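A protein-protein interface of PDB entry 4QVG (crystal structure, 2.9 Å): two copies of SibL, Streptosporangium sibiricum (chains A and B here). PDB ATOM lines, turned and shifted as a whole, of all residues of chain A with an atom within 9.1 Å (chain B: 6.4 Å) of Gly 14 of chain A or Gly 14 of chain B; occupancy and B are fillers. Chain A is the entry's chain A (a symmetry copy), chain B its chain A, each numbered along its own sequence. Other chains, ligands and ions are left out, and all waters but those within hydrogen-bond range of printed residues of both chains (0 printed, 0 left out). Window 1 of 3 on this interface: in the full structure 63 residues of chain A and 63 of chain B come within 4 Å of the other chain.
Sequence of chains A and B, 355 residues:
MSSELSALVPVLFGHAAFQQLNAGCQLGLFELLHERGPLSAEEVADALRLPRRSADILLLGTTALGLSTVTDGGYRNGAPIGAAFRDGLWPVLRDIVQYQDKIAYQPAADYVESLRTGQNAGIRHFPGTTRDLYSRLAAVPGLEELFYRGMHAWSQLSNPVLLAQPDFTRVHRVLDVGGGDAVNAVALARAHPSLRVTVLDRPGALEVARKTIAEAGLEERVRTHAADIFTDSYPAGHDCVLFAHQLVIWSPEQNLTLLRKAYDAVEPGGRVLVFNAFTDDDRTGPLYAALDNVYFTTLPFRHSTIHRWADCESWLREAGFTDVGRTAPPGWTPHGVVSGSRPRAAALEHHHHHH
Of the 23 printed residues of chain A, 17 touch a printed residue of chain B. Hydrophobic or aromatic side chains of chain A that line the printed part of chain B: Val 11, Phe 13, Ala 16, Ala 17, Phe 18, Leu 21, Tyr 105, Ala 108, Leu 287, Leu 291 and Val 294. Printed residues of chain B that touch a printed residue of chain A: Val 9, Val 11, Leu 12, Phe 13, Gly 14, His 15, Ala 16, Ala 17, Phe 18, Gln 19 and Leu 291. Hydrophobic or aromatic side chains of chain B within 4 Å of the printed part of chain A: Val 9, Val 11, Leu 12, Phe 13, His 15, Ala 16, Ala 17, Phe 18 and Leu 291. Along chain B the printed residues that touch a printed residue of chain A span positions 9 to 291. Among the printed residues, no Asp or Glu carboxylate lies within 4 Å of a Lys or Arg side-chain nitrogen of the other chain.
Phe 13 of chain A touches Leu 291 of chain B (O to CD1, 3.5 Å). Gly 14 of chain A touches His 15 of chain B. His 15 of chain A touches His 15 of chain B (CA to CA, 3.7 Å). Leu 291 of chain B touches Ala 16 of chain A (O to CB, 3.3 Å). O of Ala 17 of chain A touches CG1 of Val 11 of chain B, at 3.4 Å. Leu 21 of chain A touches Val 11 of chain B. Leu 21 of chain A touches Leu 12 of chain B (CD2 to CA, 3.8 Å). Gln 100 of chain A touches Phe 13 of chain B. His 15 of chain B touches Gln 100 of chain A (CE1 to NE2, 3.96 Å). Leu 287 of chain A touches Val 9 of chain B.
Ala 7 of chain A touches none of the printed residues of chain B. Printed residues of chain B within 4 Å of Gly 14 of chain A: Gly 14 and His 15. Of the printed residues of chain A, Val 11 of chain B touches Ala 17, Phe 18 and Leu 21. Gly 14 of chain B touches just these residues of chain A: Gly 14 and His 15. Printed residues of chain A within 4 Å of Ala 16 of chain B: Leu 291 (3.3 Å) and Val 294 (3.6 Å). Ala 17 of chain B touches just these residues of chain A: Val 11 and Leu 291.
The backbone carbonyl oxygen (O) of Leu 12 of chain B is in hydrogen-bond range of the side-chain amide nitrogen (NE2) of Gln 100 of chain A (3.3 Å). The side-chain amide nitrogen of Gln 19 of chain B sits close to the backbone carbonyl oxygen of Ala 108 of chain A, 3.4 Å away. The backbone carbonyl oxygen (O) of Gly 14 of chain A lies close to the backbone carbonyl oxygen (O) of Gly 14 of chain B (3.1 Å).
The backbone carbonyl oxygen (O) of Gln 100 of chain A is in hydrogen-bond range of the backbone NH (N) of Tyr 105 of chain A.
Val 11 of chain A touches Phe 18 of chain B, and with the chains exchanged Phe 18 of chain A touches Val 11 of chain B. Gly 14 of chain A touches His 15 of chain B, and with the chains exchanged His 15 of chain A touches Gly 14 of chain B. His 15 of chain A touches Phe 18 of chain B, and with the chains exchanged Phe 18 of chain A touches His 15 of chain B. Ala 16 of chain A touches Leu 291 of chain B, and with the chains exchanged Leu 291 of chain A touches Ala 16 of chain B. Of the 30 pairs that touch across the chains among the printed residues, 18 have their exchanged pair printed and touching as well.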
ATOM      1  N   ALA A   7     -18.724 -37.638 -25.762  1.00  0.00           N
ATOM      2  CA  ALA A   7     -18.598 -36.190 -25.879  1.00  0.00           C
ATOM      3  C   ALA A   7     -19.658 -35.633 -26.814  1.00  0.00           C
ATOM      4  O   ALA A   7     -19.893 -34.430 -26.820  1.00  0.00           O
ATOM      5  CB  ALA A   7     -17.220 -35.802 -26.351  1.00  0.00           C
ATOM      6  N   LEU A   8     -20.318 -36.501 -27.585  1.00  0.00           N
ATOM      7  CA  LEU A   8     -21.356 -36.020 -28.478  1.00  0.00           C
ATOM      8  C   LEU A   8     -22.619 -35.625 -27.752  1.00  0.00           C
ATOM      9  O   LEU A   8     -23.421 -34.872 -28.299  1.00  0.00           O
ATOM     10  CB  LEU A   8     -21.744 -37.057 -29.503  1.00  0.00           C
ATOM     11  CG  LEU A   8     -20.745 -37.298 -30.617  1.00  0.00           C
ATOM     12  CD1 LEU A   8     -21.378 -38.259 -31.621  1.00  0.00           C
ATOM     13  CD2 LEU A   8     -20.279 -35.991 -31.258  1.00  0.00           C
ATOM     14  N   VAL A   9     -22.830 -36.180 -26.558  1.00  0.00           N
ATOM     15  CA  VAL A   9     -24.108 -36.024 -25.874  1.00  0.00           C
ATOM     16  C   VAL A   9     -24.497 -34.581 -25.576  1.00  0.00           C
ATOM     17  O   VAL A   9     -25.583 -34.148 -25.981  1.00  0.00           O
ATOM     18  CB  VAL A   9     -24.203 -36.910 -24.615  1.00  0.00           C
ATOM     19  CG1 VAL A   9     -25.434 -36.549 -23.807  1.00  0.00           C
ATOM     20  CG2 VAL A   9     -24.185 -38.388 -25.004  1.00  0.00           C
ATOM     21  N   PRO A  10     -23.617 -33.812 -24.915  1.00  0.00           N
ATOM     22  CA  PRO A  10     -24.038 -32.426 -24.680  1.00  0.00           C
ATOM     23  C   PRO A  10     -24.146 -31.589 -25.946  1.00  0.00           C
ATOM     24  O   PRO A  10     -24.618 -30.465 -25.865  1.00  0.00           O
ATOM     25  CB  PRO A  10     -22.953 -31.869 -23.762  1.00  0.00           C
ATOM     26  CG  PRO A  10     -21.823 -32.810 -23.847  1.00  0.00           C
ATOM     27  CD  PRO A  10     -22.368 -34.141 -24.205  1.00  0.00           C
ATOM     28  N   VAL A  11     -23.707 -32.109 -27.086  1.00  0.00           N
ATOM     29  CA  VAL A  11     -23.797 -31.372 -28.346  1.00  0.00           C
ATOM     30  C   VAL A  11     -25.026 -31.821 -29.152  1.00  0.00           C
ATOM     31  O   VAL A  11     -25.831 -31.016 -29.594  1.00  0.00           O
ATOM     32  CB  VAL A  11     -22.529 -31.597 -29.194  1.00  0.00           C
ATOM     33  CG1 VAL A  11     -22.576 -30.763 -30.465  1.00  0.00           C
ATOM     34  CG2 VAL A  11     -21.297 -31.264 -28.388  1.00  0.00           C
ATOM     35  N   LEU A  12     -25.161 -33.123 -29.341  1.00  0.00           N
ATOM     36  CA  LEU A  12     -26.302 -33.686 -30.040  1.00  0.00           C
ATOM     37  C   LEU A  12     -27.631 -33.324 -29.353  1.00  0.00           C
ATOM     38  O   LEU A  12     -28.672 -33.194 -30.012  1.00  0.00           O
ATOM     39  CB  LEU A  12     -26.144 -35.197 -30.115  1.00  0.00           C
ATOM     40  CG  LEU A  12     -27.308 -36.058 -30.614  1.00  0.00           C
ATOM     41  CD1 LEU A  12     -27.727 -35.694 -32.022  1.00  0.00           C
ATOM     42  CD2 LEU A  12     -26.967 -37.544 -30.470  1.00  0.00           C
ATOM     43  N   PHE A  13     -27.589 -33.175 -28.027  1.00  0.00           N
ATOM     44  CA  PHE A  13     -28.754 -32.755 -27.251  1.00  0.00           C
ATOM     45  C   PHE A  13     -28.556 -31.363 -26.636  1.00  0.00           C
ATOM     46  O   PHE A  13     -29.166 -31.040 -25.598  1.00  0.00           O
ATOM     47  CB  PHE A  13     -29.018 -33.727 -26.102  1.00  0.00           C
ATOM     48  CG  PHE A  13     -29.316 -35.122 -26.528  1.00  0.00           C
ATOM     49  CD1 PHE A  13     -30.591 -35.483 -26.927  1.00  0.00           C
ATOM     50  CD2 PHE A  13     -28.316 -36.087 -26.533  1.00  0.00           C
ATOM     51  CE1 PHE A  13     -30.881 -36.799 -27.294  1.00  0.00           C
ATOM     52  CE2 PHE A  13     -28.600 -37.404 -26.917  1.00  0.00           C
ATOM     53  CZ  PHE A  13     -29.879 -37.757 -27.296  1.00  0.00           C
ATOM     54  N   GLY A  14     -27.711 -30.551 -27.263  1.00  0.00           N
ATOM     55  CA  GLY A  14     -27.347 -29.252 -26.725  1.00  0.00           C
ATOM     56  C   GLY A  14     -28.518 -28.305 -26.590  1.00  0.00           C
ATOM     57  O   GLY A  14     -28.561 -27.500 -25.658  1.00  0.00           O
ATOM     58  N   HIS A  15     -29.459 -28.389 -27.522  1.00  0.00           N
ATOM     59  CA  HIS A  15     -30.607 -27.495 -27.499  1.00  0.00           C
ATOM     60  C   HIS A  15     -31.490 -27.863 -26.328  1.00  0.00           C
ATOM     61  O   HIS A  15     -32.225 -27.036 -25.802  1.00  0.00           O
ATOM     62  CB  HIS A  15     -31.411 -27.568 -28.797  1.00  0.00           C
ATOM     63  CG  HIS A  15     -32.035 -28.902 -29.043  1.00  0.00           C
ATOM     64  ND1 HIS A  15     -31.307 -30.074 -29.069  1.00  0.00           N
ATOM     65  CD2 HIS A  15     -33.318 -29.257 -29.272  1.00  0.00           C
ATOM     66  CE1 HIS A  15     -32.114 -31.092 -29.295  1.00  0.00           C
ATOM     67  NE2 HIS A  15     -33.343 -30.624 -29.415  1.00  0.00           N
ATOM     68  N   ALA A  16     -31.494 -29.136 -25.978  1.00  0.00           N
ATOM     69  CA  ALA A  16     -32.258 -29.575 -24.832  1.00  0.00           C
ATOM     70  C   ALA A  16     -31.552 -29.120 -23.554  1.00  0.00           C
ATOM     71  O   ALA A  16     -32.203 -28.707 -22.590  1.00  0.00           O
ATOM     72  CB  ALA A  16     -32.431 -31.086 -24.865  1.00  0.00           C
ATOM     73  N   ALA A  17     -30.221 -29.198 -23.543  1.00  0.00           N
ATOM     74  CA  ALA A  17     -29.460 -28.762 -22.369  1.00  0.00           C
ATOM     75  C   ALA A  17     -29.811 -27.327 -22.056  1.00  0.00           C
ATOM     76  O   ALA A  17     -30.090 -26.994 -20.913  1.00  0.00           O
ATOM     77  CB  ALA A  17     -27.959 -28.909 -22.592  1.00  0.00           C
ATOM     78  N   PHE A  18     -29.897 -26.502 -23.086  1.00  0.00           N
ATOM     79  CA  PHE A  18     -30.290 -25.129 -22.863  1.00  0.00           C
ATOM     80  C   PHE A  18     -31.692 -25.082 -22.272  1.00  0.00           C
ATOM     81  O   PHE A  18     -31.961 -24.307 -21.362  1.00  0.00           O
ATOM     82  CB  PHE A  18     -30.278 -24.317 -24.152  1.00  0.00           C
ATOM     83  CG  PHE A  18     -30.977 -22.987 -24.023  1.00  0.00           C
ATOM     84  CD1 PHE A  18     -30.398 -21.947 -23.303  1.00  0.00           C
ATOM     85  CD2 PHE A  18     -32.240 -22.795 -24.558  1.00  0.00           C
ATOM     86  CE1 PHE A  18     -31.046 -20.725 -23.155  1.00  0.00           C
ATOM     87  CE2 PHE A  18     -32.898 -21.570 -24.412  1.00  0.00           C
ATOM     88  CZ  PHE A  18     -32.298 -20.538 -23.711  1.00  0.00           C
ATOM     89  N   GLN A  19     -32.591 -25.906 -22.785  1.00  0.00           N
ATOM     90  CA  GLN A  19     -33.961 -25.817 -22.337  1.00  0.00           C
ATOM     91  C   GLN A  19     -34.117 -26.146 -20.853  1.00  0.00           C
ATOM     92  O   GLN A  19     -35.037 -25.658 -20.196  1.00  0.00           O
ATOM     93  CB  GLN A  19     -34.883 -26.682 -23.189  1.00  0.00           C
ATOM     94  CG  GLN A  19     -35.125 -26.143 -24.582  1.00  0.00           C
ATOM     95  CD  GLN A  19     -35.727 -24.764 -24.566  1.00  0.00           C
ATOM     96  OE1 GLN A  19     -36.196 -24.296 -23.531  1.00  0.00           O
ATOM     97  NE2 GLN A  19     -35.721 -24.089 -25.721  1.00  0.00           N
ATOM     98  N   GLN A  20     -33.221 -26.963 -20.316  1.00  0.00           N
ATOM     99  CA  GLN A  20     -33.275 -27.242 -18.895  1.00  0.00           C
ATOM    100  C   GLN A  20     -33.031 -25.950 -18.115  1.00  0.00           C
ATOM    101  O   GLN A  20     -33.796 -25.623 -17.214  1.00  0.00           O
ATOM    102  CB  GLN A  20     -32.284 -28.338 -18.509  1.00  0.00           C
ATOM    103  CG  GLN A  20     -32.496 -29.666 -19.242  1.00  0.00           C
ATOM    104  CD  GLN A  20     -33.878 -30.322 -18.983  1.00  0.00           C
ATOM    105  OE1 GLN A  20     -34.660 -29.871 -18.140  1.00  0.00           O
ATOM    106  NE2 GLN A  20     -34.161 -31.411 -19.695  1.00  0.00           N
ATOM    107  N   LEU A  21     -31.990 -25.199 -18.472  1.00  0.00           N
ATOM    108  CA  LEU A  21     -31.725 -23.916 -17.834  1.00  0.00           C
ATOM    109  C   LEU A  21     -32.862 -22.938 -18.077  1.00  0.00           C
ATOM    110  O   LEU A  21     -33.324 -22.273 -17.151  1.00  0.00           O
ATOM    111  CB  LEU A  21     -30.432 -23.327 -18.361  1.00  0.00           C
ATOM    112  CG  LEU A  21     -29.992 -21.916 -17.928  1.00  0.00           C
ATOM    113  CD1 LEU A  21     -29.655 -21.856 -16.432  1.00  0.00           C
ATOM    114  CD2 LEU A  21     -28.800 -21.436 -18.777  1.00  0.00           C
ATOM    115  N   LEU A  65     -27.049 -31.912 -15.590  1.00  0.00           N
ATOM    116  CA  LEU A  65     -26.269 -30.802 -16.141  1.00  0.00           C
ATOM    117  C   LEU A  65     -25.394 -30.143 -15.078  1.00  0.00           C
ATOM    118  O   LEU A  65     -24.564 -29.244 -15.388  1.00  0.00           O
ATOM    119  CB  LEU A  65     -27.185 -29.745 -16.761  1.00  0.00           C
ATOM    120  CG  LEU A  65     -27.882 -30.134 -18.053  1.00  0.00           C
ATOM    121  CD1 LEU A  65     -28.873 -29.054 -18.455  1.00  0.00           C
ATOM    122  CD2 LEU A  65     -26.840 -30.348 -19.106  1.00  0.00           C
ATOM    123  N   GLN A 100     -31.700 -15.408 -24.713  1.00  0.00           N
ATOM    124  CA  GLN A 100     -31.512 -16.607 -25.528  1.00  0.00           C
ATOM    125  C   GLN A 100     -32.852 -17.256 -25.861  1.00  0.00           C
ATOM    126  O   GLN A 100     -33.068 -17.676 -26.982  1.00  0.00           O
ATOM    127  CB  GLN A 100     -30.599 -17.609 -24.818  1.00  0.00           C
ATOM    128  CG  GLN A 100     -29.271 -17.027 -24.302  1.00  0.00           C
ATOM    129  CD  GLN A 100     -28.261 -16.780 -25.413  1.00  0.00           C
ATOM    130  OE1 GLN A 100     -28.501 -15.992 -26.322  1.00  0.00           O
ATOM    131  NE2 GLN A 100     -27.125 -17.445 -25.336  1.00  0.00           N
ATOM    132  N   TYR A 105     -32.903 -18.226 -29.705  1.00  0.00           N
ATOM    133  CA  TYR A 105     -33.137 -19.665 -29.918  1.00  0.00           C
ATOM    134  C   TYR A 105     -33.704 -20.086 -31.274  1.00  0.00           C
ATOM    135  O   TYR A 105     -33.184 -20.980 -31.939  1.00  0.00           O
ATOM    136  CB  TYR A 105     -34.045 -20.253 -28.825  1.00  0.00           C
ATOM    137  CG  TYR A 105     -34.177 -21.767 -28.926  1.00  0.00           C
ATOM    138  CD1 TYR A 105     -33.251 -22.591 -28.310  1.00  0.00           C
ATOM    139  CD2 TYR A 105     -35.225 -22.367 -29.625  1.00  0.00           C
ATOM    140  CE1 TYR A 105     -33.340 -23.952 -28.386  1.00  0.00           C
ATOM    141  CE2 TYR A 105     -35.327 -23.750 -29.716  1.00  0.00           C
ATOM    142  CZ  TYR A 105     -34.369 -24.540 -29.097  1.00  0.00           C
ATOM    143  OH  TYR A 105     -34.422 -25.932 -29.153  1.00  0.00           O
ATOM    144  N   ALA A 108     -31.420 -19.289 -34.424  1.00  0.00           N
ATOM    145  CA  ALA A 108     -30.206 -20.104 -34.508  1.00  0.00           C
ATOM    146  C   ALA A 108     -30.354 -21.290 -35.449  1.00  0.00           C
ATOM    147  O   ALA A 108     -29.359 -21.850 -35.918  1.00  0.00           O
ATOM    148  CB  ALA A 108     -29.802 -20.586 -33.137  1.00  0.00           C
ATOM    149  N   LEU A 287     -14.687 -21.540 -25.802  1.00  0.00           N
ATOM    150  CA  LEU A 287     -16.008 -22.030 -26.207  1.00  0.00           C
ATOM    151  C   LEU A 287     -17.113 -20.941 -26.221  1.00  0.00           C
ATOM    152  O   LEU A 287     -17.899 -20.874 -27.176  1.00  0.00           O
ATOM    153  CB  LEU A 287     -16.422 -23.185 -25.288  1.00  0.00           C
ATOM    154  CG  LEU A 287     -17.709 -23.922 -25.633  1.00  0.00           C
ATOM    155  CD1 LEU A 287     -17.695 -24.443 -27.068  1.00  0.00           C
ATOM    156  CD2 LEU A 287     -17.974 -25.021 -24.647  1.00  0.00           C
ATOM    157  N   LEU A 291     -19.496 -20.247 -29.430  1.00  0.00           N
ATOM    158  CA  LEU A 291     -20.908 -20.573 -29.540  1.00  0.00           C
ATOM    159  C   LEU A 291     -21.720 -19.306 -29.671  1.00  0.00           C
ATOM    160  O   LEU A 291     -22.778 -19.296 -30.305  1.00  0.00           O
ATOM    161  CB  LEU A 291     -21.366 -21.420 -28.361  1.00  0.00           C
ATOM    162  CG  LEU A 291     -20.669 -22.779 -28.253  1.00  0.00           C
ATOM    163  CD1 LEU A 291     -21.325 -23.667 -27.173  1.00  0.00           C
ATOM    164  CD2 LEU A 291     -20.727 -23.424 -29.602  1.00  0.00           C
ATOM    165  N   ASP A 292     -21.206 -18.222 -29.104  1.00  0.00           N
ATOM    166  CA  ASP A 292     -21.835 -16.919 -29.255  1.00  0.00           C
ATOM    167  C   ASP A 292     -21.897 -16.445 -30.722  1.00  0.00           C
ATOM    168  O   ASP A 292     -22.720 -15.615 -31.084  1.00  0.00           O
ATOM    169  CB  ASP A 292     -21.082 -15.881 -28.445  1.00  0.00           C
ATOM    170  CG  ASP A 292     -21.964 -14.722 -28.041  1.00  0.00           C
ATOM    171  OD1 ASP A 292     -23.200 -14.957 -27.921  1.00  0.00           O
ATOM    172  OD2 ASP A 292     -21.438 -13.595 -27.866  1.00  0.00           O
ATOM    173  N   VAL A 294     -23.041 -17.848 -33.226  1.00  0.00           N
ATOM    174  CA  VAL A 294     -24.257 -18.245 -33.922  1.00  0.00           C
ATOM    175  C   VAL A 294     -25.246 -17.107 -33.918  1.00  0.00           C
ATOM    176  O   VAL A 294     -25.894 -16.830 -34.923  1.00  0.00           O
ATOM    177  CB  VAL A 294     -24.902 -19.489 -33.301  1.00  0.00           C
ATOM    178  CG1 VAL A 294     -26.163 -19.880 -34.055  1.00  0.00           C
ATOM    179  CG2 VAL A 294     -23.954 -20.627 -33.334  1.00  0.00           C
ATOM    180  N   LEU B   8     -21.493 -23.192 -16.977  1.00  0.00           N
ATOM    181  CA  LEU B   8     -22.709 -22.679 -17.581  1.00  0.00           C
ATOM    182  C   LEU B   8     -22.614 -22.559 -19.082  1.00  0.00           C
ATOM    183  O   LEU B   8     -23.644 -22.505 -19.750  1.00  0.00           O
ATOM    184  CB  LEU B   8     -23.069 -21.312 -17.051  1.00  0.00           C
ATOM    185  CG  LEU B   8     -23.621 -21.269 -15.640  1.00  0.00           C
ATOM    186  CD1 LEU B   8     -24.059 -19.836 -15.348  1.00  0.00           C
ATOM    187  CD2 LEU B   8     -24.742 -22.287 -15.434  1.00  0.00           C
ATOM    188  N   VAL B   9     -21.393 -22.450 -19.605  1.00  0.00           N
ATOM    189  CA  VAL B   9     -21.207 -22.124 -21.014  1.00  0.00           C
ATOM    190  C   VAL B   9     -21.830 -23.121 -21.983  1.00  0.00           C
ATOM    191  O   VAL B   9     -22.635 -22.721 -22.834  1.00  0.00           O
ATOM    192  CB  VAL B   9     -19.728 -21.848 -21.354  1.00  0.00           C
ATOM    193  CG1 VAL B   9     -19.541 -21.749 -22.856  1.00  0.00           C
ATOM    194  CG2 VAL B   9     -19.243 -20.592 -20.631  1.00  0.00           C
ATOM    195  N   PRO B  10     -21.511 -24.418 -21.849  1.00  0.00           N
ATOM    196  CA  PRO B  10     -22.162 -25.333 -22.795  1.00  0.00           C
ATOM    197  C   PRO B  10     -23.666 -25.459 -22.599  1.00  0.00           C
ATOM    198  O   PRO B  10     -24.311 -26.090 -23.422  1.00  0.00           O
ATOM    199  CB  PRO B  10     -21.475 -26.670 -22.537  1.00  0.00           C
ATOM    200  CG  PRO B  10     -20.784 -26.532 -21.243  1.00  0.00           C
ATOM    201  CD  PRO B  10     -20.479 -25.095 -21.044  1.00  0.00           C
ATOM    202  N   VAL B  11     -24.213 -24.891 -21.531  1.00  0.00           N
ATOM    203  CA  VAL B  11     -25.654 -24.954 -21.287  1.00  0.00           C
ATOM    204  C   VAL B  11     -26.340 -23.660 -21.753  1.00  0.00           C
ATOM    205  O   VAL B  11     -27.313 -23.681 -22.490  1.00  0.00           O
ATOM    206  CB  VAL B  11     -25.938 -25.162 -19.785  1.00  0.00           C
ATOM    207  CG1 VAL B  11     -27.430 -25.317 -19.536  1.00  0.00           C
ATOM    208  CG2 VAL B  11     -25.187 -26.369 -19.277  1.00  0.00           C
ATOM    209  N   LEU B  12     -25.822 -22.526 -21.309  1.00  0.00           N
ATOM    210  CA  LEU B  12     -26.341 -21.232 -21.712  1.00  0.00           C
ATOM    211  C   LEU B  12     -26.275 -21.038 -23.237  1.00  0.00           C
ATOM    212  O   LEU B  12     -27.113 -20.340 -23.826  1.00  0.00           O
ATOM    213  CB  LEU B  12     -25.551 -20.139 -21.008  1.00  0.00           C
ATOM    214  CG  LEU B  12     -25.752 -18.677 -21.416  1.00  0.00           C
ATOM    215  CD1 LEU B  12     -27.186 -18.224 -21.236  1.00  0.00           C
ATOM    216  CD2 LEU B  12     -24.758 -17.780 -20.673  1.00  0.00           C
ATOM    217  N   PHE B  13     -25.269 -21.649 -23.867  1.00  0.00           N
ATOM    218  CA  PHE B  13     -25.126 -21.618 -25.322  1.00  0.00           C
ATOM    219  C   PHE B  13     -25.332 -23.007 -25.943  1.00  0.00           C
ATOM    220  O   PHE B  13     -24.801 -23.296 -27.032  1.00  0.00           O
ATOM    221  CB  PHE B  13     -23.728 -21.146 -25.718  1.00  0.00           C
ATOM    222  CG  PHE B  13     -23.388 -19.769 -25.265  1.00  0.00           C
ATOM    223  CD1 PHE B  13     -23.802 -18.663 -25.987  1.00  0.00           C
ATOM    224  CD2 PHE B  13     -22.649 -19.572 -24.105  1.00  0.00           C
ATOM    225  CE1 PHE B  13     -23.456 -17.373 -25.582  1.00  0.00           C
ATOM    226  CE2 PHE B  13     -22.314 -18.277 -23.686  1.00  0.00           C
ATOM    227  CZ  PHE B  13     -22.716 -17.182 -24.424  1.00  0.00           C
ATOM    228  N   GLY B  14     -26.091 -23.857 -25.259  1.00  0.00           N
ATOM    229  CA  GLY B  14     -26.273 -25.235 -25.676  1.00  0.00           C
ATOM    230  C   GLY B  14     -26.936 -25.374 -27.028  1.00  0.00           C
ATOM    231  O   GLY B  14     -26.623 -26.299 -27.780  1.00  0.00           O
ATOM    232  N   HIS B  15     -27.858 -24.469 -27.332  1.00  0.00           N
ATOM    233  CA  HIS B  15     -28.578 -24.541 -28.595  1.00  0.00           C
ATOM    234  C   HIS B  15     -27.625 -24.202 -29.720  1.00  0.00           C
ATOM    235  O   HIS B  15     -27.808 -24.625 -30.856  1.00  0.00           O
ATOM    236  CB  HIS B  15     -29.771 -23.587 -28.623  1.00  0.00           C
ATOM    237  CG  HIS B  15     -29.391 -22.145 -28.539  1.00  0.00           C
ATOM    238  ND1 HIS B  15     -28.618 -21.635 -27.516  1.00  0.00           N
ATOM    239  CD2 HIS B  15     -29.672 -21.100 -29.348  1.00  0.00           C
ATOM    240  CE1 HIS B  15     -28.433 -20.343 -27.703  1.00  0.00           C
ATOM    241  NE2 HIS B  15     -29.057 -19.994 -28.814  1.00  0.00           N
ATOM    242  N   ALA B  16     -26.655 -23.355 -29.429  1.00  0.00           N
ATOM    243  CA  ALA B  16     -25.659 -23.018 -30.421  1.00  0.00           C
ATOM    244  C   ALA B  16     -24.709 -24.204 -30.599  1.00  0.00           C
ATOM    245  O   ALA B  16     -24.294 -24.513 -31.720  1.00  0.00           O
ATOM    246  CB  ALA B  16     -24.910 -21.762 -30.005  1.00  0.00           C
ATOM    247  N   ALA B  17     -24.360 -24.866 -29.496  1.00  0.00           N
ATOM    248  CA  ALA B  17     -23.472 -26.029 -29.575  1.00  0.00           C
ATOM    249  C   ALA B  17     -24.070 -27.046 -30.517  1.00  0.00           C
ATOM    250  O   ALA B  17     -23.384 -27.558 -31.390  1.00  0.00           O
ATOM    251  CB  ALA B  17     -23.239 -26.646 -28.201  1.00  0.00           C
ATOM    252  N   PHE B  18     -25.371 -27.259 -30.408  1.00  0.00           N
ATOM    253  CA  PHE B  18     -26.018 -28.174 -31.322  1.00  0.00           C
ATOM    254  C   PHE B  18     -25.876 -27.666 -32.749  1.00  0.00           C
ATOM    255  O   PHE B  18     -25.616 -28.437 -33.664  1.00  0.00           O
ATOM    256  CB  PHE B  18     -27.500 -28.338 -31.008  1.00  0.00           C
ATOM    257  CG  PHE B  18     -28.268 -29.021 -32.111  1.00  0.00           C
ATOM    258  CD1 PHE B  18     -28.114 -30.384 -32.345  1.00  0.00           C
ATOM    259  CD2 PHE B  18     -29.088 -28.296 -32.959  1.00  0.00           C
ATOM    260  CE1 PHE B  18     -28.798 -31.019 -33.378  1.00  0.00           C
ATOM    261  CE2 PHE B  18     -29.776 -28.926 -33.999  1.00  0.00           C
ATOM    262  CZ  PHE B  18     -29.630 -30.288 -34.204  1.00  0.00           C
ATOM    263  N   GLN B  19     -26.049 -26.369 -32.948  1.00  0.00           N
ATOM    264  CA  GLN B  19     -26.039 -25.858 -34.298  1.00  0.00           C
ATOM    265  C   GLN B  19     -24.692 -26.055 -34.992  1.00  0.00           C
ATOM    266  O   GLN B  19     -24.627 -26.166 -36.217  1.00  0.00           O
ATOM    267  CB  GLN B  19     -26.471 -24.397 -34.345  1.00  0.00           C
ATOM    268  CG  GLN B  19     -27.947 -24.179 -34.092  1.00  0.00           C
ATOM    269  CD  GLN B  19     -28.812 -24.911 -35.082  1.00  0.00           C
ATOM    270  OE1 GLN B  19     -28.328 -25.386 -36.108  1.00  0.00           O
ATOM    271  NE2 GLN B  19     -30.112 -25.015 -34.786  1.00  0.00           N
ATOM    272  N   LEU B 291     -31.572 -35.365 -21.276  1.00  0.00           N
ATOM    273  CA  LEU B 291     -31.801 -34.317 -22.256  1.00  0.00           C
ATOM    274  C   LEU B 291     -32.772 -34.798 -23.309  1.00  0.00           C
ATOM    275  O   LEU B 291     -33.528 -34.008 -23.878  1.00  0.00           O
ATOM    276  CB  LEU B 291     -30.489 -33.846 -22.868  1.00  0.00           C
ATOM    277  CG  LEU B 291     -29.513 -33.224 -21.866  1.00  0.00           C
ATOM    278  CD1 LEU B 291     -28.304 -32.580 -22.578  1.00  0.00           C
ATOM    279  CD2 LEU B 291     -30.274 -32.219 -21.060  1.00  0.00           C
